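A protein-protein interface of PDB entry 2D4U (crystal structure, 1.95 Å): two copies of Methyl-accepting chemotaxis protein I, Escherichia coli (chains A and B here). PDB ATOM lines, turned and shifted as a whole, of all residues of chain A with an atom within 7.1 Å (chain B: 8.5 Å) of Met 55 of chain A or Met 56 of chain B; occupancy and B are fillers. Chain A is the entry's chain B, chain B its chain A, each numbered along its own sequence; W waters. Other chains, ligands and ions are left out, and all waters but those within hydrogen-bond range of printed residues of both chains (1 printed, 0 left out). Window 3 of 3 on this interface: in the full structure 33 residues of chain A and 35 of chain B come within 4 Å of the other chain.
The backbone NH (N) of Ile 61 of chain B is in hydrogen-bond range of the backbone carbonyl oxygen (O) of Met 56 of chain B (3.3 Å). The backbone carbonyl oxygen (O) of Met 56 of chain A lies within hydrogen-bond range of the backbone NH (N) of Ile 61 of chain A.
Among the printed residues, merely in contact across the chains: Asn 48 of chain A with Arg 49 of chain B (3.6 Å), Asn 48 of chain A with Ile 52 of chain B (3.6 Å), Arg 49 of chain A with Asn 48 of chain B (3.8 Å), Ile 52 of chain A with Asn 48 of chain B (3.3 Å), Ile 52 of chain A with Ile 52 of chain B (3.6 Å), Ile 52 of chain A with Met 55 of chain B (3.7 Å), Ile 52 of chain A with Phe 132 of chain B (3.7 Å), Met 55 of chain A with Ile 52 of chain B (3.5 Å), Met 55 of chain A with Met 55 of chain B (3.2 Å), Met 55 of chain A with Met 56 of chain B (3.6 Å), Met 56 of chain A with Met 55 of chain B (3.6 Å), Met 56 of chain A with Phe 132 of chain B (3.9 Å) and Phe 132 of chain A with Met 56 of chain B (3.6 Å).
Met 55 of chain A touches just these residues of chain B: Ile 52, Met 55 and Met 56. Printed residues of chain A within 4 Å of Met 55 of chain B: Ile 52 (3.7 Å), Met 55 (3.2 Å) and Met 56 (3.6 Å). Of the printed residues of chain B, Phe 132 of chain A touches Met 56. Of the printed residues of chain B, Ile 52 of chain A touches Asn 48, Ile 52, Met 55 and Phe 132. Printed residues of chain A within 4 Å of Arg 49 of chain B: Asn 48 (3.6 Å). Ala 50 of chain B touches none of the printed residues of chain A. Asp 57 of chain A touches none of the printed residues of chain B. The nearest residue of chain B that does not touch Met 55 of chain A is Gly 51 of chain B (4.9 Å). The nearest printed residue of chain B that does not touch Asn 48 of chain A is Asn 48 of chain B (4.3 Å).
Of the 18 printed residues of chain A, 6 touch a printed residue of chain B. Among the printed residues, 13 pairs touch across the chains. Among the printed residues, no Asp or Glu carboxylate lies within 4 Å of a Lys or Arg side-chain nitrogen of the other chain.
Asn 48 of chain A touches Arg 49 of chain B, and with the chains exchanged Arg 49 of chain A touches Asn 48 of chain B. Ile 52 of chain A touches Met 55 of chain B, and with the chains exchanged Met 55 of chain A touches Ile 52 of chain B. Met 55 of chain A touches Met 56 of chain B, and with the chains exchanged Met 56 of chain A touches Met 55 of chain B. Met 56 of chain A touches Phe 132 of chain B, and with the chains exchanged Phe 132 of chain A touches Met 56 of chain B. Positions printed for both chains: 48, 49, 50, 51, 52, 53, 54, 55, 56, 57, 58, 59, 60, 61, 62, 67 and 132.
Water W1 lies within hydrogen-bond range of the backbone carbonyl oxygen (O) of Met 55 of chain B and the side-chain sulfur (SD) of Met 55 of chain A.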
ATOM      1  N   ASN A  48      17.865 -24.862 -29.541  1.00  0.00           N
ATOM      2  CA  ASN A  48      17.398 -24.604 -28.170  1.00  0.00           C
ATOM      3  C   ASN A  48      16.047 -23.882 -28.217  1.00  0.00           C
ATOM      4  O   ASN A  48      15.196 -24.136 -27.385  1.00  0.00           O
ATOM      5  CB  ASN A  48      18.452 -23.854 -27.308  1.00  0.00           C
ATOM      6  CG  ASN A  48      19.597 -24.767 -26.833  1.00  0.00           C
ATOM      7  OD1 ASN A  48      19.369 -25.938 -26.489  1.00  0.00           O
ATOM      8  ND2 ASN A  48      20.823 -24.250 -26.819  1.00  0.00           N
ATOM      9  N   ARG A  49      15.816 -22.999 -29.186  1.00  0.00           N
ATOM     10  CA  ARG A  49      14.481 -22.400 -29.315  1.00  0.00           C
ATOM     11  C   ARG A  49      13.395 -23.460 -29.621  1.00  0.00           C
ATOM     12  O   ARG A  49      12.231 -23.411 -29.108  1.00  0.00           O
ATOM     13  CB  ARG A  49      14.465 -21.282 -30.353  1.00  0.00           C
ATOM     14  CG  ARG A  49      15.283 -20.039 -29.914  1.00  0.00           C
ATOM     15  CD  ARG A  49      15.347 -18.933 -30.932  1.00  0.00           C
ATOM     16  NE  ARG A  49      14.033 -18.426 -31.327  1.00  0.00           N
ATOM     17  CZ  ARG A  49      13.719 -18.156 -32.586  1.00  0.00           C
ATOM     18  NH1 ARG A  49      14.599 -18.380 -33.551  1.00  0.00           N
ATOM     19  NH2 ARG A  49      12.526 -17.701 -32.895  1.00  0.00           N
ATOM     20  N   ALA A  50      13.767 -24.427 -30.438  1.00  0.00           N
ATOM     21  CA  ALA A  50      12.854 -25.489 -30.745  1.00  0.00           C
ATOM     22  C   ALA A  50      12.564 -26.310 -29.473  1.00  0.00           C
ATOM     23  O   ALA A  50      11.437 -26.756 -29.277  1.00  0.00           O
ATOM     24  CB  ALA A  50      13.416 -26.364 -31.884  1.00  0.00           C
ATOM     25  N   GLY A  51      13.561 -26.458 -28.606  1.00  0.00           N
ATOM     26  CA  GLY A  51      13.417 -27.201 -27.364  1.00  0.00           C
ATOM     27  C   GLY A  51      12.418 -26.505 -26.446  1.00  0.00           C
ATOM     28  O   GLY A  51      11.485 -27.130 -25.929  1.00  0.00           O
ATOM     29  N   ILE A  52      12.640 -25.214 -26.219  1.00  0.00           N
ATOM     30  CA  ILE A  52      11.712 -24.391 -25.480  1.00  0.00           C
ATOM     31  C   ILE A  52      10.311 -24.521 -26.094  1.00  0.00           C
ATOM     32  O   ILE A  52       9.351 -24.804 -25.380  1.00  0.00           O
ATOM     33  CB  ILE A  52      12.168 -22.920 -25.520  1.00  0.00           C
ATOM     34  CG1 ILE A  52      13.485 -22.754 -24.779  1.00  0.00           C
ATOM     35  CG2 ILE A  52      11.086 -21.999 -24.939  1.00  0.00           C
ATOM     36  CD1 ILE A  52      14.002 -21.293 -24.751  1.00  0.00           C
ATOM     37  N   ARG A  53      10.197 -24.348 -27.412  1.00  0.00           N
ATOM     38  CA  ARG A  53       8.895 -24.403 -28.044  1.00  0.00           C
ATOM     39  C   ARG A  53       8.206 -25.738 -27.771  1.00  0.00           C
ATOM     40  O   ARG A  53       7.023 -25.768 -27.431  1.00  0.00           O
ATOM     41  CB  ARG A  53       8.961 -24.103 -29.552  1.00  0.00           C
ATOM     42  CG  ARG A  53       7.615 -24.198 -30.271  1.00  0.00           C
ATOM     43  CD  ARG A  53       6.524 -23.285 -29.719  1.00  0.00           C
ATOM     44  NE  ARG A  53       5.228 -23.804 -30.120  1.00  0.00           N
ATOM     45  CZ  ARG A  53       4.519 -23.346 -31.129  1.00  0.00           C
ATOM     46  NH1 ARG A  53       4.945 -22.286 -31.813  1.00  0.00           N
ATOM     47  NH2 ARG A  53       3.369 -23.934 -31.431  1.00  0.00           N
ATOM     48  N   TYR A  54       8.948 -26.823 -27.886  1.00  0.00           N
ATOM     49  CA  TYR A  54       8.369 -28.128 -27.641  1.00  0.00           C
ATOM     50  C   TYR A  54       7.808 -28.253 -26.236  1.00  0.00           C
ATOM     51  O   TYR A  54       6.711 -28.777 -26.059  1.00  0.00           O
ATOM     52  CB  TYR A  54       9.412 -29.220 -27.859  1.00  0.00           C
ATOM     53  CG  TYR A  54       8.944 -30.601 -27.456  1.00  0.00           C
ATOM     54  CD1 TYR A  54       8.406 -31.468 -28.394  1.00  0.00           C
ATOM     55  CD2 TYR A  54       9.030 -31.034 -26.131  1.00  0.00           C
ATOM     56  CE1 TYR A  54       7.977 -32.741 -28.031  1.00  0.00           C
ATOM     57  CE2 TYR A  54       8.596 -32.293 -25.759  1.00  0.00           C
ATOM     58  CZ  TYR A  54       8.076 -33.140 -26.716  1.00  0.00           C
ATOM     59  OH  TYR A  54       7.644 -34.387 -26.350  1.00  0.00           O
ATOM     60  N   MET A  55       8.587 -27.791 -25.256  1.00  0.00           N
ATOM     61  CA  MET A  55       8.224 -27.829 -23.842  1.00  0.00           C
ATOM     62  C   MET A  55       7.003 -26.953 -23.547  1.00  0.00           C
ATOM     63  O   MET A  55       6.172 -27.306 -22.706  1.00  0.00           O
ATOM     64  CB  MET A  55       9.410 -27.404 -22.975  1.00  0.00           C
ATOM     65  CG  MET A  55      10.605 -28.348 -23.041  1.00  0.00           C
ATOM     66  SD  MET A  55      11.487 -28.358 -21.482  1.00  0.00           S
ATOM     67  CE  MET A  55      12.728 -27.173 -21.697  1.00  0.00           C
ATOM     68  N   MET A  56       6.909 -25.813 -24.234  1.00  0.00           N
ATOM     69  CA  MET A  56       5.749 -24.931 -24.142  1.00  0.00           C
ATOM     70  C   MET A  56       4.517 -25.616 -24.737  1.00  0.00           C
ATOM     71  O   MET A  56       3.398 -25.438 -24.253  1.00  0.00           O
ATOM     72  CB  MET A  56       6.008 -23.606 -24.864  1.00  0.00           C
ATOM     73  CG  MET A  56       7.054 -22.754 -24.177  1.00  0.00           C
ATOM     74  SD  MET A  56       6.441 -22.247 -22.596  1.00  0.00           S
ATOM     75  CE  MET A  56       7.631 -21.313 -21.928  1.00  0.00           C
ATOM     76  N   ASP A  57       4.723 -26.393 -25.796  1.00  0.00           N
ATOM     77  CA  ASP A  57       3.636 -27.129 -26.423  1.00  0.00           C
ATOM     78  C   ASP A  57       3.088 -28.179 -25.473  1.00  0.00           C
ATOM     79  O   ASP A  57       1.894 -28.473 -25.493  1.00  0.00           O
ATOM     80  CB  ASP A  57       4.112 -27.831 -27.691  1.00  0.00           C
ATOM     81  CG  ASP A  57       4.283 -26.895 -28.844  1.00  0.00           C
ATOM     82  OD1 ASP A  57       3.767 -25.763 -28.766  1.00  0.00           O
ATOM     83  OD2 ASP A  57       4.911 -27.233 -29.880  1.00  0.00           O
ATOM     84  N   GLN A  58       3.968 -28.749 -24.653  1.00  0.00           N
ATOM     85  CA  GLN A  58       3.556 -29.739 -23.660  1.00  0.00           C
ATOM     86  C   GLN A  58       2.644 -29.153 -22.575  1.00  0.00           C
ATOM     87  O   GLN A  58       1.784 -29.847 -22.043  1.00  0.00           O
ATOM     88  CB  GLN A  58       4.777 -30.391 -23.013  1.00  0.00           C
ATOM     89  CG  GLN A  58       5.128 -31.731 -23.616  1.00  0.00           C
ATOM     90  CD  GLN A  58       4.646 -31.864 -25.056  1.00  0.00           C
ATOM     91  OE1 GLN A  58       3.903 -32.789 -25.385  1.00  0.00           O
ATOM     92  NE2 GLN A  58       5.060 -30.937 -25.911  1.00  0.00           N
ATOM     93  N   ASN A  59       2.854 -27.886 -22.235  1.00  0.00           N
ATOM     94  CA  ASN A  59       2.009 -27.206 -21.261  1.00  0.00           C
ATOM     95  C   ASN A  59       0.914 -26.415 -21.945  1.00  0.00           C
ATOM     96  O   ASN A  59       0.368 -25.472 -21.382  1.00  0.00           O
ATOM     97  CB  ASN A  59       2.823 -26.314 -20.333  1.00  0.00           C
ATOM     98  CG  ASN A  59       3.257 -27.036 -19.069  1.00  0.00           C
ATOM     99  OD1 ASN A  59       3.448 -28.248 -19.066  1.00  0.00           O
ATOM    100  ND2 ASN A  59       3.390 -26.289 -17.974  1.00  0.00           N
ATOM    101  N   ASN A  60       0.634 -26.814 -23.180  1.00  0.00           N
ATOM    102  CA  ASN A  60      -0.459 -26.287 -24.001  1.00  0.00           C
ATOM    103  C   ASN A  60      -0.473 -24.806 -24.299  1.00  0.00           C
ATOM    104  O   ASN A  60      -1.471 -24.275 -24.781  1.00  0.00           O
ATOM    105  CB  ASN A  60      -1.815 -26.720 -23.442  1.00  0.00           C
ATOM    106  CG  ASN A  60      -2.042 -28.197 -23.585  1.00  0.00           C
ATOM    107  OD1 ASN A  60      -1.938 -28.950 -22.612  1.00  0.00           O
ATOM    108  ND2 ASN A  60      -2.341 -28.635 -24.812  1.00  0.00           N
ATOM    109  N   ILE A  61       0.634 -24.139 -24.006  1.00  0.00           N
ATOM    110  CA  ILE A  61       0.792 -22.744 -24.354  1.00  0.00           C
ATOM    111  C   ILE A  61       1.773 -22.796 -25.522  1.00  0.00           C
ATOM    112  O   ILE A  61       1.730 -23.737 -26.306  1.00  0.00           O
ATOM    113  CB  ILE A  61       1.299 -21.977 -23.146  1.00  0.00           C
ATOM    114  CG1 ILE A  61       2.423 -22.744 -22.468  1.00  0.00           C
ATOM    115  CG2 ILE A  61       0.160 -21.807 -22.135  1.00  0.00           C
ATOM    116  CD1 ILE A  61       2.941 -22.069 -21.205  1.00  0.00           C
ATOM    117  N   GLY A  62       2.660 -21.843 -25.705  1.00  0.00           N
ATOM    118  CA  GLY A  62       3.559 -22.090 -26.820  1.00  0.00           C
ATOM    119  C   GLY A  62       3.167 -21.272 -28.021  1.00  0.00           C
ATOM    120  O   GLY A  62       2.085 -21.426 -28.600  1.00  0.00           O
ATOM    121  N   VAL A  67       7.961 -25.887 -33.658  1.00  0.00           N
ATOM    122  CA  VAL A  67       9.136 -26.719 -33.528  1.00  0.00           C
ATOM    123  C   VAL A  67       9.614 -27.081 -34.926  1.00  0.00           C
ATOM    124  O   VAL A  67      10.805 -27.054 -35.209  1.00  0.00           O
ATOM    125  CB  VAL A  67       8.818 -27.992 -32.732  1.00  0.00           C
ATOM    126  CG1 VAL A  67      10.006 -28.917 -32.701  1.00  0.00           C
ATOM    127  CG2 VAL A  67       8.374 -27.641 -31.296  1.00  0.00           C
ATOM    128  N   ILE A 128      13.092 -36.961 -28.576  1.00  0.00           N
ATOM    129  CA  ILE A 128      13.237 -35.835 -27.674  1.00  0.00           C
ATOM    130  C   ILE A 128      14.211 -36.022 -26.521  1.00  0.00           C
ATOM    131  O   ILE A 128      14.938 -35.096 -26.170  1.00  0.00           O
ATOM    132  CB  ILE A 128      11.864 -35.461 -27.105  1.00  0.00           C
ATOM    133  CG1 ILE A 128      11.968 -34.191 -26.270  1.00  0.00           C
ATOM    134  CG2 ILE A 128      11.308 -36.585 -26.264  1.00  0.00           C
ATOM    135  CD1 ILE A 128      11.453 -32.984 -26.979  1.00  0.00           C
ATOM    136  N   PHE A 132      17.510 -33.555 -25.864  1.00  0.00           N
ATOM    137  CA  PHE A 132      17.826 -32.756 -24.693  1.00  0.00           C
ATOM    138  C   PHE A 132      19.056 -33.288 -23.958  1.00  0.00           C
ATOM    139  O   PHE A 132      19.699 -32.567 -23.206  1.00  0.00           O
ATOM    140  CB  PHE A 132      16.631 -32.714 -23.742  1.00  0.00           C
ATOM    141  CG  PHE A 132      15.536 -31.772 -24.164  1.00  0.00           C
ATOM    142  CD1 PHE A 132      14.311 -32.252 -24.579  1.00  0.00           C
ATOM    143  CD2 PHE A 132      15.727 -30.407 -24.127  1.00  0.00           C
ATOM    144  CE1 PHE A 132      13.306 -31.385 -24.955  1.00  0.00           C
ATOM    145  CE2 PHE A 132      14.716 -29.528 -24.502  1.00  0.00           C
ATOM    146  CZ  PHE A 132      13.518 -30.017 -24.914  1.00  0.00           C
ATOM    147  N   ASN B  48      18.916 -18.982 -23.382  1.00  0.00           N
ATOM    148  CA  ASN B  48      17.917 -19.964 -23.779  1.00  0.00           C
ATOM    149  C   ASN B  48      18.123 -21.287 -23.044  1.00  0.00           C
ATOM    150  O   ASN B  48      17.144 -21.925 -22.681  1.00  0.00           O
ATOM    151  CB  ASN B  48      17.833 -20.150 -25.298  1.00  0.00           C
ATOM    152  CG  ASN B  48      17.000 -19.073 -25.959  1.00  0.00           C
ATOM    153  OD1 ASN B  48      15.948 -18.679 -25.442  1.00  0.00           O
ATOM    154  ND2 ASN B  48      17.461 -18.586 -27.094  1.00  0.00           N
ATOM    155  N   ARG B  49      19.371 -21.688 -22.839  1.00  0.00           N
ATOM    156  CA  ARG B  49      19.700 -22.895 -22.088  1.00  0.00           C
ATOM    157  C   ARG B  49      19.205 -22.760 -20.655  1.00  0.00           C
ATOM    158  O   ARG B  49      18.722 -23.728 -20.064  1.00  0.00           O
ATOM    159  CB  ARG B  49      21.212 -23.150 -22.068  1.00  0.00           C
ATOM    160  CG  ARG B  49      21.798 -23.673 -23.388  1.00  0.00           C
ATOM    161  CD  ARG B  49      23.330 -23.778 -23.370  1.00  0.00           C
ATOM    162  NE  ARG B  49      23.852 -24.634 -22.297  1.00  0.00           N
ATOM    163  CZ  ARG B  49      25.046 -24.466 -21.724  1.00  0.00           C
ATOM    164  NH1 ARG B  49      25.842 -23.478 -22.105  1.00  0.00           N
ATOM    165  NH2 ARG B  49      25.452 -25.277 -20.768  1.00  0.00           N
ATOM    166  N   ALA B  50      19.332 -21.566 -20.109  1.00  0.00           N
ATOM    167  CA  ALA B  50      18.825 -21.285 -18.763  1.00  0.00           C
ATOM    168  C   ALA B  50      17.283 -21.459 -18.676  1.00  0.00           C
ATOM    169  O   ALA B  50      16.739 -22.016 -17.704  1.00  0.00           O
ATOM    170  CB  ALA B  50      19.257 -19.918 -18.321  1.00  0.00           C
ATOM    171  N   GLY B  51      16.576 -21.031 -19.709  1.00  0.00           N
ATOM    172  CA  GLY B  51      15.133 -21.165 -19.736  1.00  0.00           C
ATOM    173  C   GLY B  51      14.738 -22.635 -19.821  1.00  0.00           C
ATOM    174  O   GLY B  51      13.743 -23.072 -19.231  1.00  0.00           O
ATOM    175  N   ILE B  52      15.512 -23.404 -20.568  1.00  0.00           N
ATOM    176  CA  ILE B  52      15.241 -24.829 -20.702  1.00  0.00           C
ATOM    177  C   ILE B  52      15.471 -25.513 -19.351  1.00  0.00           C
ATOM    178  O   ILE B  52      14.626 -26.274 -18.881  1.00  0.00           O
ATOM    179  CB  ILE B  52      16.172 -25.435 -21.745  1.00  0.00           C
ATOM    180  CG1 ILE B  52      15.630 -25.176 -23.144  1.00  0.00           C
ATOM    181  CG2 ILE B  52      16.388 -26.912 -21.511  1.00  0.00           C
ATOM    182  CD1 ILE B  52      16.607 -25.556 -24.229  1.00  0.00           C
ATOM    183  N   ARG B  53      16.623 -25.245 -18.749  1.00  0.00           N
ATOM    184  CA  ARG B  53      16.949 -25.834 -17.464  1.00  0.00           C
ATOM    185  C   ARG B  53      15.858 -25.497 -16.457  1.00  0.00           C
ATOM    186  O   ARG B  53      15.515 -26.325 -15.620  1.00  0.00           O
ATOM    187  CB  ARG B  53      18.313 -25.353 -16.966  1.00  0.00           C
ATOM    188  CG  ARG B  53      18.709 -25.876 -15.564  1.00  0.00           C
ATOM    189  CD  ARG B  53      18.800 -27.389 -15.447  1.00  0.00           C
ATOM    190  NE  ARG B  53      18.651 -27.836 -14.059  1.00  0.00           N
ATOM    191  CZ  ARG B  53      19.652 -28.171 -13.240  1.00  0.00           C
ATOM    192  NH1 ARG B  53      20.919 -28.109 -13.631  1.00  0.00           N
ATOM    193  NH2 ARG B  53      19.383 -28.562 -12.004  1.00  0.00           N
ATOM    194  N   TYR B  54      15.304 -24.295 -16.555  1.00  0.00           N
ATOM    195  CA  TYR B  54      14.239 -23.873 -15.645  1.00  0.00           C
ATOM    196  C   TYR B  54      13.007 -24.742 -15.840  1.00  0.00           C
ATOM    197  O   TYR B  54      12.450 -25.245 -14.865  1.00  0.00           O
ATOM    198  CB  TYR B  54      13.864 -22.391 -15.815  1.00  0.00           C
ATOM    199  CG  TYR B  54      12.783 -21.942 -14.851  1.00  0.00           C
ATOM    200  CD1 TYR B  54      11.452 -21.875 -15.248  1.00  0.00           C
ATOM    201  CD2 TYR B  54      13.093 -21.600 -13.539  1.00  0.00           C
ATOM    202  CE1 TYR B  54      10.464 -21.467 -14.366  1.00  0.00           C
ATOM    203  CE2 TYR B  54      12.107 -21.187 -12.650  1.00  0.00           C
ATOM    204  CZ  TYR B  54      10.795 -21.124 -13.073  1.00  0.00           C
ATOM    205  OH  TYR B  54       9.799 -20.722 -12.195  1.00  0.00           O
ATOM    206  N   MET B  55      12.594 -24.908 -17.099  1.00  0.00           N
ATOM    207  CA  MET B  55      11.402 -25.675 -17.444  1.00  0.00           C
ATOM    208  C   MET B  55      11.609 -27.157 -17.135  1.00  0.00           C
ATOM    209  O   MET B  55      10.652 -27.903 -16.941  1.00  0.00           O
ATOM    210  CB  MET B  55      11.037 -25.484 -18.920  1.00  0.00           C
ATOM    211  CG  MET B  55      10.279 -24.179 -19.250  1.00  0.00           C
ATOM    212  SD  MET B  55       9.853 -24.023 -21.025  1.00  0.00           S
ATOM    213  CE  MET B  55      11.468 -24.186 -21.793  1.00  0.00           C
ATOM    214  N   MET B  56      12.865 -27.583 -17.117  1.00  0.00           N
ATOM    215  CA  MET B  56      13.186 -28.962 -16.793  1.00  0.00           C
ATOM    216  C   MET B  56      13.119 -29.144 -15.298  1.00  0.00           C
ATOM    217  O   MET B  56      12.696 -30.189 -14.813  1.00  0.00           O
ATOM    218  CB  MET B  56      14.594 -29.302 -17.257  1.00  0.00           C
ATOM    219  CG  MET B  56      14.752 -29.371 -18.755  1.00  0.00           C
ATOM    220  SD  MET B  56      14.701 -31.026 -19.326  1.00  0.00           S
ATOM    221  CE  MET B  56      14.028 -30.841 -20.964  1.00  0.00           C
ATOM    222  N   ASP B  57      13.550 -28.120 -14.570  1.00  0.00           N
ATOM    223  CA  ASP B  57      13.592 -28.181 -13.119  1.00  0.00           C
ATOM    224  C   ASP B  57      12.192 -28.211 -12.549  1.00  0.00           C
ATOM    225  O   ASP B  57      12.007 -28.587 -11.397  1.00  0.00           O
ATOM    226  CB  ASP B  57      14.327 -26.983 -12.512  1.00  0.00           C
ATOM    227  CG  ASP B  57      15.851 -27.093 -12.604  1.00  0.00           C
ATOM    228  OD1 ASP B  57      16.391 -28.204 -12.769  1.00  0.00           O
ATOM    229  OD2 ASP B  57      16.599 -26.093 -12.513  1.00  0.00           O
ATOM    230  N   GLN B  58      11.212 -27.776 -13.332  1.00  0.00           N
ATOM    231  CA  GLN B  58       9.839 -27.740 -12.839  1.00  0.00           C
ATOM    232  C   GLN B  58       9.389 -29.158 -12.509  1.00  0.00           C
ATOM    233  O   GLN B  58       8.721 -29.401 -11.502  1.00  0.00           O
ATOM    234  CB  GLN B  58       8.894 -27.111 -13.870  1.00  0.00           C
ATOM    235  CG  GLN B  58       9.290 -25.708 -14.330  1.00  0.00           C
ATOM    236  CD  GLN B  58       9.274 -24.691 -13.200  1.00  0.00           C
ATOM    237  OE1 GLN B  58      10.317 -24.383 -12.608  1.00  0.00           O
ATOM    238  NE2 GLN B  58       8.096 -24.153 -12.911  1.00  0.00           N
ATOM    239  N   ASN B  59       9.764 -30.095 -13.365  1.00  0.00           N
ATOM    240  CA  ASN B  59       9.406 -31.488 -13.171  1.00  0.00           C
ATOM    241  C   ASN B  59      10.567 -32.241 -12.549  1.00  0.00           C
ATOM    242  O   ASN B  59      10.848 -33.378 -12.899  1.00  0.00           O
ATOM    243  CB  ASN B  59       8.984 -32.087 -14.510  1.00  0.00           C
ATOM    244  CG  ASN B  59       8.160 -31.116 -15.325  1.00  0.00           C
ATOM    245  OD1 ASN B  59       7.640 -30.140 -14.779  1.00  0.00           O
ATOM    246  ND2 ASN B  59       8.054 -31.355 -16.633  1.00  0.00           N
ATOM    247  N   ASN B  60      11.233 -31.567 -11.617  1.00  0.00           N
ATOM    248  CA  ASN B  60      12.384 -32.083 -10.870  1.00  0.00           C
ATOM    249  C   ASN B  60      13.446 -32.858 -11.647  1.00  0.00           C
ATOM    250  O   ASN B  60      14.317 -33.507 -11.056  1.00  0.00           O
ATOM    251  CB  ASN B  60      11.952 -32.821  -9.594  1.00  0.00           C
ATOM    252  CG  ASN B  60      11.741 -31.866  -8.413  1.00  0.00           C
ATOM    253  OD1 ASN B  60      12.411 -31.971  -7.377  1.00  0.00           O
ATOM    254  ND2 ASN B  60      10.826 -30.918  -8.578  1.00  0.00           N
ATOM    255  N   ILE B  61      13.388 -32.791 -12.972  1.00  0.00           N
ATOM    256  CA  ILE B  61      14.442 -33.390 -13.765  1.00  0.00           C
ATOM    257  C   ILE B  61      15.357 -32.225 -14.142  1.00  0.00           C
ATOM    258  O   ILE B  61      15.442 -31.253 -13.386  1.00  0.00           O
ATOM    259  CB  ILE B  61      13.893 -34.196 -14.971  1.00  0.00           C
ATOM    260  CG1 ILE B  61      13.366 -33.289 -16.075  1.00  0.00           C
ATOM    261  CG2 ILE B  61      12.801 -35.159 -14.515  1.00  0.00           C
ATOM    262  CD1 ILE B  61      13.118 -34.018 -17.374  1.00  0.00           C
ATOM    263  N   GLY B  62      16.048 -32.278 -15.270  1.00  0.00           N
ATOM    264  CA  GLY B  62      16.900 -31.147 -15.568  1.00  0.00           C
ATOM    265  C   GLY B  62      18.233 -31.421 -14.920  1.00  0.00           C
ATOM    266  O   GLY B  62      18.325 -31.761 -13.735  1.00  0.00           O
ATOM    267  N   SER B  63      19.275 -31.302 -15.729  1.00  0.00           N
ATOM    268  CA  SER B  63      20.623 -31.618 -15.306  1.00  0.00           C
ATOM    269  C   SER B  63      21.565 -30.619 -15.936  1.00  0.00           C
ATOM    270  O   SER B  63      21.126 -29.621 -16.501  1.00  0.00           O
ATOM    271  CB  SER B  63      20.984 -33.023 -15.782  1.00  0.00           C
ATOM    272  OG  SER B  63      20.461 -33.248 -17.086  1.00  0.00           O
ATOM    273  N   SER B  65      24.280 -27.663 -16.149  1.00  0.00           N
ATOM    274  CA  SER B  65      24.481 -26.416 -15.453  1.00  0.00           C
ATOM    275  C   SER B  65      23.175 -25.943 -14.841  1.00  0.00           C
ATOM    276  O   SER B  65      22.103 -26.162 -15.401  1.00  0.00           O
ATOM    277  CB  SER B  65      24.949 -25.351 -16.456  1.00  0.00           C
ATOM    278  OG  SER B  65      26.210 -25.690 -16.994  1.00  0.00           O
ATOM    279  N   VAL B  67      20.432 -22.976 -13.456  1.00  0.00           N
ATOM    280  CA  VAL B  67      19.936 -21.703 -13.918  1.00  0.00           C
ATOM    281  C   VAL B  67      20.900 -20.612 -13.461  1.00  0.00           C
ATOM    282  O   VAL B  67      21.349 -19.788 -14.263  1.00  0.00           O
ATOM    283  CB  VAL B  67      18.520 -21.452 -13.386  1.00  0.00           C
ATOM    284  CG1 VAL B  67      17.997 -20.102 -13.838  1.00  0.00           C
ATOM    285  CG2 VAL B  67      17.584 -22.542 -13.867  1.00  0.00           C
ATOM    286  N   PHE B 132      10.418 -15.180 -21.157  1.00  0.00           N
ATOM    287  CA  PHE B 132      10.124 -16.014 -22.313  1.00  0.00           C
ATOM    288  C   PHE B 132       9.510 -15.240 -23.470  1.00  0.00           C
ATOM    289  O   PHE B 132       9.640 -15.611 -24.635  1.00  0.00           O
ATOM    290  CB  PHE B 132       9.285 -17.237 -21.894  1.00  0.00           C
ATOM    291  CG  PHE B 132      10.126 -18.387 -21.402  1.00  0.00           C
ATOM    292  CD1 PHE B 132      10.158 -18.744 -20.061  1.00  0.00           C
ATOM    293  CD2 PHE B 132      10.922 -19.085 -22.281  1.00  0.00           C
ATOM    294  CE1 PHE B 132      10.946 -19.775 -19.620  1.00  0.00           C
ATOM    295  CE2 PHE B 132      11.707 -20.117 -21.837  1.00  0.00           C
ATOM    296  CZ  PHE B 132      11.720 -20.451 -20.501  1.00  0.00           C
HETATM  297  O   HOH W   1       9.757 -29.175 -19.119  1.00  0.00           O
